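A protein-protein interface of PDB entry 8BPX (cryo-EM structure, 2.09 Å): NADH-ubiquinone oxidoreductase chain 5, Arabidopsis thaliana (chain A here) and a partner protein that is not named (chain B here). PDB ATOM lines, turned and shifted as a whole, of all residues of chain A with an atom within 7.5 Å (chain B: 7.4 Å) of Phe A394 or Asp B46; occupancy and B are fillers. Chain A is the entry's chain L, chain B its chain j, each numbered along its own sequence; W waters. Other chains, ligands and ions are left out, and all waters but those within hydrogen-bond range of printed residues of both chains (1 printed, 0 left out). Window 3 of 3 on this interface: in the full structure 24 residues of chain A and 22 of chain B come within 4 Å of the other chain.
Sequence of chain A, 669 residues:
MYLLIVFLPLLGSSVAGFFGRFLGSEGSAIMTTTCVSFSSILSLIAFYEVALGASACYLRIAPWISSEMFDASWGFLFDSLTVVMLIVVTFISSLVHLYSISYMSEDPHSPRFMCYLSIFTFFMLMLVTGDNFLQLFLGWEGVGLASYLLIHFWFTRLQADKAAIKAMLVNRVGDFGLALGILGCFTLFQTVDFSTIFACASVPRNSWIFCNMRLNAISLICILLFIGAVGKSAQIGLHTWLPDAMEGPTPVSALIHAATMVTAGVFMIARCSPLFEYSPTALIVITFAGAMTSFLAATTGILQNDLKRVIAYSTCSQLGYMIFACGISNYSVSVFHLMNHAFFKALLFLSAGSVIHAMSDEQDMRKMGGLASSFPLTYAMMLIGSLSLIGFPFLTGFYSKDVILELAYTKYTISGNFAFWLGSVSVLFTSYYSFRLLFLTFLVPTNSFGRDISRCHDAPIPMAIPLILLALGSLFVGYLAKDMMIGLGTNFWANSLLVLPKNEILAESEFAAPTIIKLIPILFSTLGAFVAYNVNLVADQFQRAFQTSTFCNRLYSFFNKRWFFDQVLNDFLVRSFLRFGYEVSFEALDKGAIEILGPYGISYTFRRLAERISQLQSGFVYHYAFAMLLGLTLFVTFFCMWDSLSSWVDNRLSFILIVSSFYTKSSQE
O of Phe A394 lies within hydrogen-bond range of NE1 of Trp B38.
The guanidinium group (NE) of Arg B42 lies within salt-bridge range of the side-chain carboxylate (OD2) of Asp B46 (2.9 Å).
Among the printed residues, pairs that only touch across the chains: Phe A392 with Ile B39, Phe A394 with Ile B39, Phe A394 with Arg B42, Phe A394 with Ala B43, Phe A394 with Asp B46, Tyr A399 with Arg B42, Leu A475 with Trp B38, Phe A476 with Trp B38, Tyr A479 with Trp B38 and Tyr A479 with Arg B42.
Phe A394 touches just these residues of chain B: Trp B38 (3.1 Å), Ile B39 (3.9 Å), Arg B42 (3.5 Å), Ala B43 (3.6 Å) and Asp B46 (3.1 Å). Of chain A, only Phe A394 (3.1 Å) comes within 4 Å of Asp B46. Printed residues of chain B within 4 Å of Phe A392: Ile B39 (3.5 Å). Of the printed residues of chain A, Arg B42 touches Phe A394 (3.5 Å), Tyr A399 (3.4 Å) and Tyr A479 (3.5 Å). Printed residues of chain A within 4 Å of Trp B38: Phe A394, Leu A475, Phe A476 and Tyr A479. Of the printed residues of chain B, Leu A475 touches Trp B38. Printed residues of chain A within 4 Å of Ile B39: Phe A392 (3.5 Å) and Phe A394 (3.9 Å). Pro A393 touches none of the printed residues of chain B. The nearest printed residue of chain B that does not touch Phe A394 is Gly B47 (4.7 Å).
Printed residues of chain B that touch a printed residue of chain A: Trp B38, Ile B39, Arg B42, Ala B43 and Asp B46. Hydrophobic or aromatic side chains of chain B that line the printed part of chain A: Trp B38, Ile B39 and Ala B43. Of the 16 printed residues of chain A, 6 touch a printed residue of chain B. Printed residues of chain A that touch a printed residue of chain B: Phe A392, Phe A394, Tyr A399, Leu A475, Phe A476 and Tyr A479. Among the printed residues, 11 pairs touch across the chains.
Water W1 bridges OH of Tyr A399 and OD1 of Asp B46.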
ATOM      1  N   GLY A 391     -19.726  10.849  16.018  1.00  0.00           N
ATOM      2  CA  GLY A 391     -19.977  11.497  17.289  1.00  0.00           C
ATOM      3  C   GLY A 391     -20.832  10.680  18.236  1.00  0.00           C
ATOM      4  O   GLY A 391     -21.651  11.239  18.969  1.00  0.00           O
ATOM      5  N   PHE A 392     -20.663   9.364  18.221  1.00  0.00           N
ATOM      6  CA  PHE A 392     -21.354   8.520  19.184  1.00  0.00           C
ATOM      7  C   PHE A 392     -20.942   8.915  20.600  1.00  0.00           C
ATOM      8  O   PHE A 392     -19.754   9.132  20.862  1.00  0.00           O
ATOM      9  CB  PHE A 392     -21.043   7.044  18.938  1.00  0.00           C
ATOM     10  CG  PHE A 392     -22.066   6.102  19.522  1.00  0.00           C
ATOM     11  CD1 PHE A 392     -21.974   5.692  20.841  1.00  0.00           C
ATOM     12  CD2 PHE A 392     -23.122   5.641  18.756  1.00  0.00           C
ATOM     13  CE1 PHE A 392     -22.916   4.834  21.388  1.00  0.00           C
ATOM     14  CE2 PHE A 392     -24.062   4.780  19.291  1.00  0.00           C
ATOM     15  CZ  PHE A 392     -23.959   4.375  20.610  1.00  0.00           C
ATOM     16  N   PRO A 393     -21.891   9.011  21.529  1.00  0.00           N
ATOM     17  CA  PRO A 393     -21.590   9.561  22.857  1.00  0.00           C
ATOM     18  C   PRO A 393     -20.411   8.885  23.540  1.00  0.00           C
ATOM     19  O   PRO A 393     -20.282   7.660  23.543  1.00  0.00           O
ATOM     20  CB  PRO A 393     -22.893   9.332  23.627  1.00  0.00           C
ATOM     21  CG  PRO A 393     -23.947   9.406  22.578  1.00  0.00           C
ATOM     22  CD  PRO A 393     -23.339   8.842  21.315  1.00  0.00           C
ATOM     23  N   PHE A 394     -19.534   9.716  24.105  1.00  0.00           N
ATOM     24  CA  PHE A 394     -18.390   9.368  24.941  1.00  0.00           C
ATOM     25  C   PHE A 394     -17.248   8.710  24.174  1.00  0.00           C
ATOM     26  O   PHE A 394     -16.244   8.347  24.786  1.00  0.00           O
ATOM     27  CB  PHE A 394     -18.809   8.490  26.129  1.00  0.00           C
ATOM     28  CG  PHE A 394     -20.091   8.934  26.762  1.00  0.00           C
ATOM     29  CD1 PHE A 394     -20.165  10.155  27.411  1.00  0.00           C
ATOM     30  CD2 PHE A 394     -21.232   8.155  26.681  1.00  0.00           C
ATOM     31  CE1 PHE A 394     -21.349  10.583  27.975  1.00  0.00           C
ATOM     32  CE2 PHE A 394     -22.411   8.577  27.248  1.00  0.00           C
ATOM     33  CZ  PHE A 394     -22.468   9.791  27.898  1.00  0.00           C
ATOM     34  N   LEU A 395     -17.358   8.562  22.862  1.00  0.00           N
ATOM     35  CA  LEU A 395     -16.226   8.181  22.036  1.00  0.00           C
ATOM     36  C   LEU A 395     -15.425   9.434  21.684  1.00  0.00           C
ATOM     37  O   LEU A 395     -15.840  10.560  21.958  1.00  0.00           O
ATOM     38  CB  LEU A 395     -16.708   7.449  20.785  1.00  0.00           C
ATOM     39  CG  LEU A 395     -17.262   6.035  20.990  1.00  0.00           C
ATOM     40  CD1 LEU A 395     -17.141   5.217  19.717  1.00  0.00           C
ATOM     41  CD2 LEU A 395     -16.558   5.338  22.145  1.00  0.00           C
ATOM     42  N   THR A 396     -14.263   9.232  21.058  1.00  0.00           N
ATOM     43  CA  THR A 396     -13.311  10.329  20.898  1.00  0.00           C
ATOM     44  C   THR A 396     -13.904  11.489  20.105  1.00  0.00           C
ATOM     45  O   THR A 396     -13.755  12.651  20.496  1.00  0.00           O
ATOM     46  CB  THR A 396     -12.028   9.821  20.240  1.00  0.00           C
ATOM     47  OG1 THR A 396     -11.269   9.078  21.197  1.00  0.00           O
ATOM     48  CG2 THR A 396     -11.185  10.970  19.723  1.00  0.00           C
ATOM     49  N   GLY A 397     -14.610  11.198  19.012  1.00  0.00           N
ATOM     50  CA  GLY A 397     -15.184  12.262  18.206  1.00  0.00           C
ATOM     51  C   GLY A 397     -16.340  12.996  18.857  1.00  0.00           C
ATOM     52  O   GLY A 397     -16.685  14.095  18.419  1.00  0.00           O
ATOM     53  N   PHE A 398     -16.942  12.411  19.894  1.00  0.00           N
ATOM     54  CA  PHE A 398     -18.056  13.045  20.596  1.00  0.00           C
ATOM     55  C   PHE A 398     -17.624  14.301  21.347  1.00  0.00           C
ATOM     56  O   PHE A 398     -18.406  15.247  21.465  1.00  0.00           O
ATOM     57  CB  PHE A 398     -18.689  12.028  21.551  1.00  0.00           C
ATOM     58  CG  PHE A 398     -19.654  12.618  22.550  1.00  0.00           C
ATOM     59  CD1 PHE A 398     -19.223  13.008  23.810  1.00  0.00           C
ATOM     60  CD2 PHE A 398     -20.992  12.764  22.237  1.00  0.00           C
ATOM     61  CE1 PHE A 398     -20.114  13.535  24.730  1.00  0.00           C
ATOM     62  CE2 PHE A 398     -21.882  13.291  23.150  1.00  0.00           C
ATOM     63  CZ  PHE A 398     -21.445  13.674  24.399  1.00  0.00           C
ATOM     64  N   TYR A 399     -16.465  14.325  21.941  1.00  0.00           N
ATOM     65  CA  TYR A 399     -16.040  15.450  22.792  1.00  0.00           C
ATOM     66  C   TYR A 399     -15.670  16.748  22.028  1.00  0.00           C
ATOM     67  O   TYR A 399     -15.626  17.778  22.658  1.00  0.00           O
ATOM     68  CB  TYR A 399     -14.884  14.976  23.671  1.00  0.00           C
ATOM     69  CG  TYR A 399     -15.278  13.939  24.680  1.00  0.00           C
ATOM     70  CD1 TYR A 399     -15.908  14.313  25.856  1.00  0.00           C
ATOM     71  CD2 TYR A 399     -15.072  12.593  24.442  1.00  0.00           C
ATOM     72  CE1 TYR A 399     -16.303  13.371  26.784  1.00  0.00           C
ATOM     73  CE2 TYR A 399     -15.461  11.641  25.362  1.00  0.00           C
ATOM     74  CZ  TYR A 399     -16.065  12.036  26.543  1.00  0.00           C
ATOM     75  OH  TYR A 399     -16.459  11.116  27.459  1.00  0.00           O
ATOM     76  N   ASP A 402     -19.501  17.947  18.986  1.00  0.00           N
ATOM     77  CA  ASP A 402     -20.679  18.561  19.585  1.00  0.00           C
ATOM     78  C   ASP A 402     -20.342  19.856  20.303  1.00  0.00           C
ATOM     79  O   ASP A 402     -21.175  20.763  20.354  1.00  0.00           O
ATOM     80  CB  ASP A 402     -21.361  17.577  20.527  1.00  0.00           C
ATOM     81  CG  ASP A 402     -21.317  16.166  20.009  1.00  0.00           C
ATOM     82  OD1 ASP A 402     -21.014  15.258  20.798  1.00  0.00           O
ATOM     83  OD2 ASP A 402     -21.581  15.962  18.807  1.00  0.00           O
ATOM     84  N   SER A 474      -9.090   6.140  19.224  1.00  0.00           N
ATOM     85  CA  SER A 474     -10.438   6.549  18.859  1.00  0.00           C
ATOM     86  C   SER A 474     -11.463   6.236  19.938  1.00  0.00           C
ATOM     87  O   SER A 474     -12.571   6.776  19.888  1.00  0.00           O
ATOM     88  CB  SER A 474     -10.848   5.874  17.548  1.00  0.00           C
ATOM     89  OG  SER A 474      -9.893   6.117  16.528  1.00  0.00           O
ATOM     90  N   LEU A 475     -11.140   5.361  20.885  1.00  0.00           N
ATOM     91  CA  LEU A 475     -12.020   5.168  22.031  1.00  0.00           C
ATOM     92  C   LEU A 475     -11.738   6.133  23.172  1.00  0.00           C
ATOM     93  O   LEU A 475     -12.682   6.652  23.772  1.00  0.00           O
ATOM     94  CB  LEU A 475     -11.929   3.734  22.562  1.00  0.00           C
ATOM     95  CG  LEU A 475     -12.397   2.619  21.629  1.00  0.00           C
ATOM     96  CD1 LEU A 475     -12.043   1.263  22.209  1.00  0.00           C
ATOM     97  CD2 LEU A 475     -13.879   2.736  21.346  1.00  0.00           C
ATOM     98  N   PHE A 476     -10.469   6.405  23.484  1.00  0.00           N
ATOM     99  CA  PHE A 476     -10.143   7.026  24.761  1.00  0.00           C
ATOM    100  C   PHE A 476      -9.498   8.407  24.697  1.00  0.00           C
ATOM    101  O   PHE A 476      -9.497   9.104  25.719  1.00  0.00           O
ATOM    102  CB  PHE A 476      -9.232   6.097  25.576  1.00  0.00           C
ATOM    103  CG  PHE A 476      -9.832   4.752  25.825  1.00  0.00           C
ATOM    104  CD1 PHE A 476     -11.052   4.640  26.474  1.00  0.00           C
ATOM    105  CD2 PHE A 476      -9.198   3.599  25.396  1.00  0.00           C
ATOM    106  CE1 PHE A 476     -11.619   3.404  26.697  1.00  0.00           C
ATOM    107  CE2 PHE A 476      -9.761   2.361  25.622  1.00  0.00           C
ATOM    108  CZ  PHE A 476     -10.973   2.265  26.273  1.00  0.00           C
ATOM    109  N   VAL A 477      -8.965   8.831  23.549  1.00  0.00           N
ATOM    110  CA  VAL A 477      -8.162  10.046  23.513  1.00  0.00           C
ATOM    111  C   VAL A 477      -9.017  11.276  23.788  1.00  0.00           C
ATOM    112  O   VAL A 477      -8.592  12.193  24.502  1.00  0.00           O
ATOM    113  CB  VAL A 477      -7.424  10.148  22.165  1.00  0.00           C
ATOM    114  CG1 VAL A 477      -7.094  11.591  21.835  1.00  0.00           C
ATOM    115  CG2 VAL A 477      -6.166   9.297  22.197  1.00  0.00           C
ATOM    116  N   GLY A 478     -10.238  11.337  23.274  1.00  0.00           N
ATOM    117  CA  GLY A 478     -11.135  12.467  23.508  1.00  0.00           C
ATOM    118  C   GLY A 478     -11.388  12.768  24.978  1.00  0.00           C
ATOM    119  O   GLY A 478     -11.115  13.845  25.388  1.00  0.00           O
ATOM    120  N   TYR A 479     -11.961  11.808  25.690  1.00  0.00           N
ATOM    121  CA  TYR A 479     -12.197  11.888  27.134  1.00  0.00           C
ATOM    122  C   TYR A 479     -10.923  12.245  27.840  1.00  0.00           C
ATOM    123  O   TYR A 479     -10.945  13.189  28.578  1.00  0.00           O
ATOM    124  CB  TYR A 479     -12.708  10.547  27.650  1.00  0.00           C
ATOM    125  CG  TYR A 479     -12.665  10.428  29.145  1.00  0.00           C
ATOM    126  CD1 TYR A 479     -13.632  11.037  29.925  1.00  0.00           C
ATOM    127  CD2 TYR A 479     -11.637   9.753  29.776  1.00  0.00           C
ATOM    128  CE1 TYR A 479     -13.605  10.936  31.301  1.00  0.00           C
ATOM    129  CE2 TYR A 479     -11.597   9.642  31.151  1.00  0.00           C
ATOM    130  CZ  TYR A 479     -12.583  10.235  31.913  1.00  0.00           C
ATOM    131  OH  TYR A 479     -12.521  10.163  33.266  1.00  0.00           O
ATOM    132  N   TRP B  38     -17.253   0.720  27.956  1.00  0.00           N
ATOM    133  CA  TRP B  38     -16.844   2.098  28.182  1.00  0.00           C
ATOM    134  C   TRP B  38     -18.008   3.053  27.966  1.00  0.00           C
ATOM    135  O   TRP B  38     -18.197   3.998  28.740  1.00  0.00           O
ATOM    136  CB  TRP B  38     -15.673   2.434  27.260  1.00  0.00           C
ATOM    137  CG  TRP B  38     -15.325   3.877  27.176  1.00  0.00           C
ATOM    138  CD1 TRP B  38     -15.629   4.729  26.162  1.00  0.00           C
ATOM    139  CD2 TRP B  38     -14.589   4.641  28.135  1.00  0.00           C
ATOM    140  NE1 TRP B  38     -15.128   5.979  26.426  1.00  0.00           N
ATOM    141  CE2 TRP B  38     -14.487   5.952  27.634  1.00  0.00           C
ATOM    142  CE3 TRP B  38     -14.015   4.345  29.373  1.00  0.00           C
ATOM    143  CZ2 TRP B  38     -13.829   6.963  28.327  1.00  0.00           C
ATOM    144  CZ3 TRP B  38     -13.360   5.351  30.055  1.00  0.00           C
ATOM    145  CH2 TRP B  38     -13.275   6.644  29.532  1.00  0.00           C
ATOM    146  N   ILE B  39     -18.808   2.812  26.927  1.00  0.00           N
ATOM    147  CA  ILE B  39     -19.972   3.657  26.685  1.00  0.00           C
ATOM    148  C   ILE B  39     -20.960   3.555  27.841  1.00  0.00           C
ATOM    149  O   ILE B  39     -21.491   4.566  28.309  1.00  0.00           O
ATOM    150  CB  ILE B  39     -20.626   3.293  25.340  1.00  0.00           C
ATOM    151  CG1 ILE B  39     -19.734   3.737  24.179  1.00  0.00           C
ATOM    152  CG2 ILE B  39     -22.012   3.923  25.223  1.00  0.00           C
ATOM    153  CD1 ILE B  39     -20.148   3.171  22.847  1.00  0.00           C
ATOM    154  N   LEU B  40     -21.221   2.336  28.322  1.00  0.00           N
ATOM    155  CA  LEU B  40     -22.169   2.168  29.423  1.00  0.00           C
ATOM    156  C   LEU B  40     -21.675   2.849  30.695  1.00  0.00           C
ATOM    157  O   LEU B  40     -22.437   3.551  31.374  1.00  0.00           O
ATOM    158  CB  LEU B  40     -22.416   0.682  29.671  1.00  0.00           C
ATOM    159  CG  LEU B  40     -23.204  -0.039  28.579  1.00  0.00           C
ATOM    160  CD1 LEU B  40     -23.327  -1.516  28.893  1.00  0.00           C
ATOM    161  CD2 LEU B  40     -24.573   0.594  28.386  1.00  0.00           C
ATOM    162  N   TYR B  41     -20.397   2.662  31.021  1.00  0.00           N
ATOM    163  CA  TYR B  41     -19.822   3.264  32.217  1.00  0.00           C
ATOM    164  C   TYR B  41     -19.856   4.784  32.136  1.00  0.00           C
ATOM    165  O   TYR B  41     -20.252   5.460  33.096  1.00  0.00           O
ATOM    166  CB  TYR B  41     -18.393   2.749  32.401  1.00  0.00           C
ATOM    167  CG  TYR B  41     -17.673   3.254  33.631  1.00  0.00           C
ATOM    168  CD1 TYR B  41     -17.004   4.471  33.616  1.00  0.00           C
ATOM    169  CD2 TYR B  41     -17.652   2.508  34.802  1.00  0.00           C
ATOM    170  CE1 TYR B  41     -16.339   4.932  34.725  1.00  0.00           C
ATOM    171  CE2 TYR B  41     -16.993   2.966  35.919  1.00  0.00           C
ATOM    172  CZ  TYR B  41     -16.336   4.179  35.873  1.00  0.00           C
ATOM    173  OH  TYR B  41     -15.677   4.645  36.982  1.00  0.00           O
ATOM    174  N   ARG B  42     -19.461   5.342  30.987  1.00  0.00           N
ATOM    175  CA  ARG B  42     -19.478   6.789  30.820  1.00  0.00           C
ATOM    176  C   ARG B  42     -20.897   7.330  30.888  1.00  0.00           C
ATOM    177  O   ARG B  42     -21.131   8.403  31.455  1.00  0.00           O
ATOM    178  CB  ARG B  42     -18.829   7.177  29.493  1.00  0.00           C
ATOM    179  CG  ARG B  42     -17.318   7.188  29.515  1.00  0.00           C
ATOM    180  CD  ARG B  42     -16.777   8.591  29.681  1.00  0.00           C
ATOM    181  NE  ARG B  42     -16.919   9.079  31.048  1.00  0.00           N
ATOM    182  CZ  ARG B  42     -16.199   8.654  32.078  1.00  0.00           C
ATOM    183  NH1 ARG B  42     -15.284   7.710  31.940  1.00  0.00           N
ATOM    184  NH2 ARG B  42     -16.400   9.194  33.275  1.00  0.00           N
ATOM    185  N   ALA B  43     -21.854   6.614  30.297  1.00  0.00           N
ATOM    186  CA  ALA B  43     -23.240   7.049  30.361  1.00  0.00           C
ATOM    187  C   ALA B  43     -23.712   7.111  31.805  1.00  0.00           C
ATOM    188  O   ALA B  43     -24.244   8.130  32.244  1.00  0.00           O
ATOM    189  CB  ALA B  43     -24.124   6.120  29.531  1.00  0.00           C
ATOM    190  N   LYS B  44     -23.445   6.061  32.579  1.00  0.00           N
ATOM    191  CA  LYS B  44     -23.841   6.083  33.983  1.00  0.00           C
ATOM    192  C   LYS B  44     -23.158   7.217  34.745  1.00  0.00           C
ATOM    193  O   LYS B  44     -23.799   7.897  35.555  1.00  0.00           O
ATOM    194  CB  LYS B  44     -23.542   4.735  34.633  1.00  0.00           C
ATOM    195  CG  LYS B  44     -23.194   4.819  36.097  1.00  0.00           C
ATOM    196  CD  LYS B  44     -23.864   3.710  36.876  1.00  0.00           C
ATOM    197  CE  LYS B  44     -23.173   3.500  38.201  1.00  0.00           C
ATOM    198  NZ  LYS B  44     -21.737   3.180  37.985  1.00  0.00           N
ATOM    199  N   GLN B  45     -21.869   7.451  34.493  1.00  0.00           N
ATOM    200  CA  GLN B  45     -21.141   8.451  35.271  1.00  0.00           C
ATOM    201  C   GLN B  45     -21.594   9.868  34.938  1.00  0.00           C
ATOM    202  O   GLN B  45     -21.849  10.672  35.840  1.00  0.00           O
ATOM    203  CB  GLN B  45     -19.636   8.316  35.055  1.00  0.00           C
ATOM    204  CG  GLN B  45     -18.990   7.206  35.853  1.00  0.00           C
ATOM    205  CD  GLN B  45     -18.776   7.587  37.301  1.00  0.00           C
ATOM    206  OE1 GLN B  45     -19.320   6.954  38.205  1.00  0.00           O
ATOM    207  NE2 GLN B  45     -17.989   8.630  37.529  1.00  0.00           N
ATOM    208  N   ASP B  46     -21.695  10.202  33.653  1.00  0.00           N
ATOM    209  CA  ASP B  46     -21.948  11.587  33.272  1.00  0.00           C
ATOM    210  C   ASP B  46     -22.998  11.681  32.175  1.00  0.00           C
ATOM    211  O   ASP B  46     -22.831  12.414  31.197  1.00  0.00           O
ATOM    212  CB  ASP B  46     -20.654  12.284  32.847  1.00  0.00           C
ATOM    213  CG  ASP B  46     -19.828  11.452  31.901  1.00  0.00           C
ATOM    214  OD1 ASP B  46     -20.310  11.164  30.787  1.00  0.00           O
ATOM    215  OD2 ASP B  46     -18.694  11.081  32.268  1.00  0.00           O
ATOM    216  N   GLY B  47     -24.104  10.963  32.325  1.00  0.00           N
ATOM    217  CA  GLY B  47     -25.220  11.085  31.423  1.00  0.00           C
ATOM    218  C   GLY B  47     -26.346  11.962  31.935  1.00  0.00           C
ATOM    219  O   GLY B  47     -27.006  12.650  31.154  1.00  0.00           O
ATOM    220  N   PRO B  48     -26.574  11.941  33.292  1.00  0.00           N
ATOM    221  CA  PRO B  48     -27.533  12.859  33.860  1.00  0.00           C
ATOM    222  C   PRO B  48     -26.990  14.264  33.609  1.00  0.00           C
ATOM    223  O   PRO B  48     -27.789  15.126  33.428  1.00  0.00           O
ATOM    224  CB  PRO B  48     -27.649  12.431  35.312  1.00  0.00           C
ATOM    225  CG  PRO B  48     -27.276  10.991  35.287  1.00  0.00           C
ATOM    226  CD  PRO B  48     -26.107  11.009  34.344  1.00  0.00           C
ATOM    227  N   VAL B  49     -25.675  14.450  33.557  1.00  0.00           N
ATOM    228  CA  VAL B  49     -25.226  15.870  33.355  1.00  0.00           C
ATOM    229  C   VAL B  49     -25.551  16.354  31.936  1.00  0.00           C
ATOM    230  O   VAL B  49     -26.103  17.430  31.828  1.00  0.00           O
ATOM    231  CB  VAL B  49     -23.781  16.118  33.806  1.00  0.00           C
ATOM    232  CG1 VAL B  49     -23.211  17.411  33.253  1.00  0.00           C
ATOM    233  CG2 VAL B  49     -23.644  16.068  35.314  1.00  0.00           C
ATOM    234  N   VAL B  50     -25.290  15.545  30.903  1.00  0.00           N
ATOM    235  CA  VAL B  50     -25.570  15.892  29.511  1.00  0.00           C
ATOM    236  C   VAL B  50     -27.073  15.970  29.274  1.00  0.00           C
ATOM    237  O   VAL B  50     -27.547  16.766  28.455  1.00  0.00           O
ATOM    238  CB  VAL B  50     -24.880  14.903  28.546  1.00  0.00           C
ATOM    239  CG1 VAL B  50     -23.462  14.620  29.003  1.00  0.00           C
ATOM    240  CG2 VAL B  50     -25.658  13.610  28.423  1.00  0.00           C
ATOM    241  N   MET B  51     -27.846  15.059  29.901  1.00  0.00           N
ATOM    242  CA  MET B  51     -29.325  15.154  29.818  1.00  0.00           C
ATOM    243  C   MET B  51     -29.784  16.454  30.466  1.00  0.00           C
ATOM    244  O   MET B  51     -30.909  16.867  30.177  1.00  0.00           O
ATOM    245  CB  MET B  51     -30.038  14.002  30.544  1.00  0.00           C
ATOM    246  CG  MET B  51     -31.088  13.348  29.694  1.00  0.00           C
ATOM    247  SD  MET B  51     -30.506  13.256  27.992  1.00  0.00           S
ATOM    248  CE  MET B  51     -29.248  11.990  28.176  1.00  0.00           C
ATOM    249  N   ARG B  54     -29.080  17.050  36.306  1.00  0.00           N
ATOM    250  CA  ARG B  54     -28.292  17.693  37.370  1.00  0.00           C
ATOM    251  C   ARG B  54     -27.033  18.433  36.887  1.00  0.00           C
ATOM    252  O   ARG B  54     -26.735  18.405  35.718  1.00  0.00           O
ATOM    253  CB  ARG B  54     -27.785  16.637  38.336  1.00  0.00           C
ATOM    254  CG  ARG B  54     -27.021  15.513  37.651  1.00  0.00           C
ATOM    255  CD  ARG B  54     -26.507  14.494  38.630  1.00  0.00           C
ATOM    256  NE  ARG B  54     -25.655  15.148  39.600  1.00  0.00           N
ATOM    257  CZ  ARG B  54     -24.345  15.297  39.466  1.00  0.00           C
ATOM    258  NH1 ARG B  54     -23.734  14.835  38.392  1.00  0.00           N
ATOM    259  NH2 ARG B  54     -23.656  15.921  40.400  1.00  0.00           N
HETATM  260  O   HOH W   1     -17.904  12.403  29.413  1.00  0.00           O
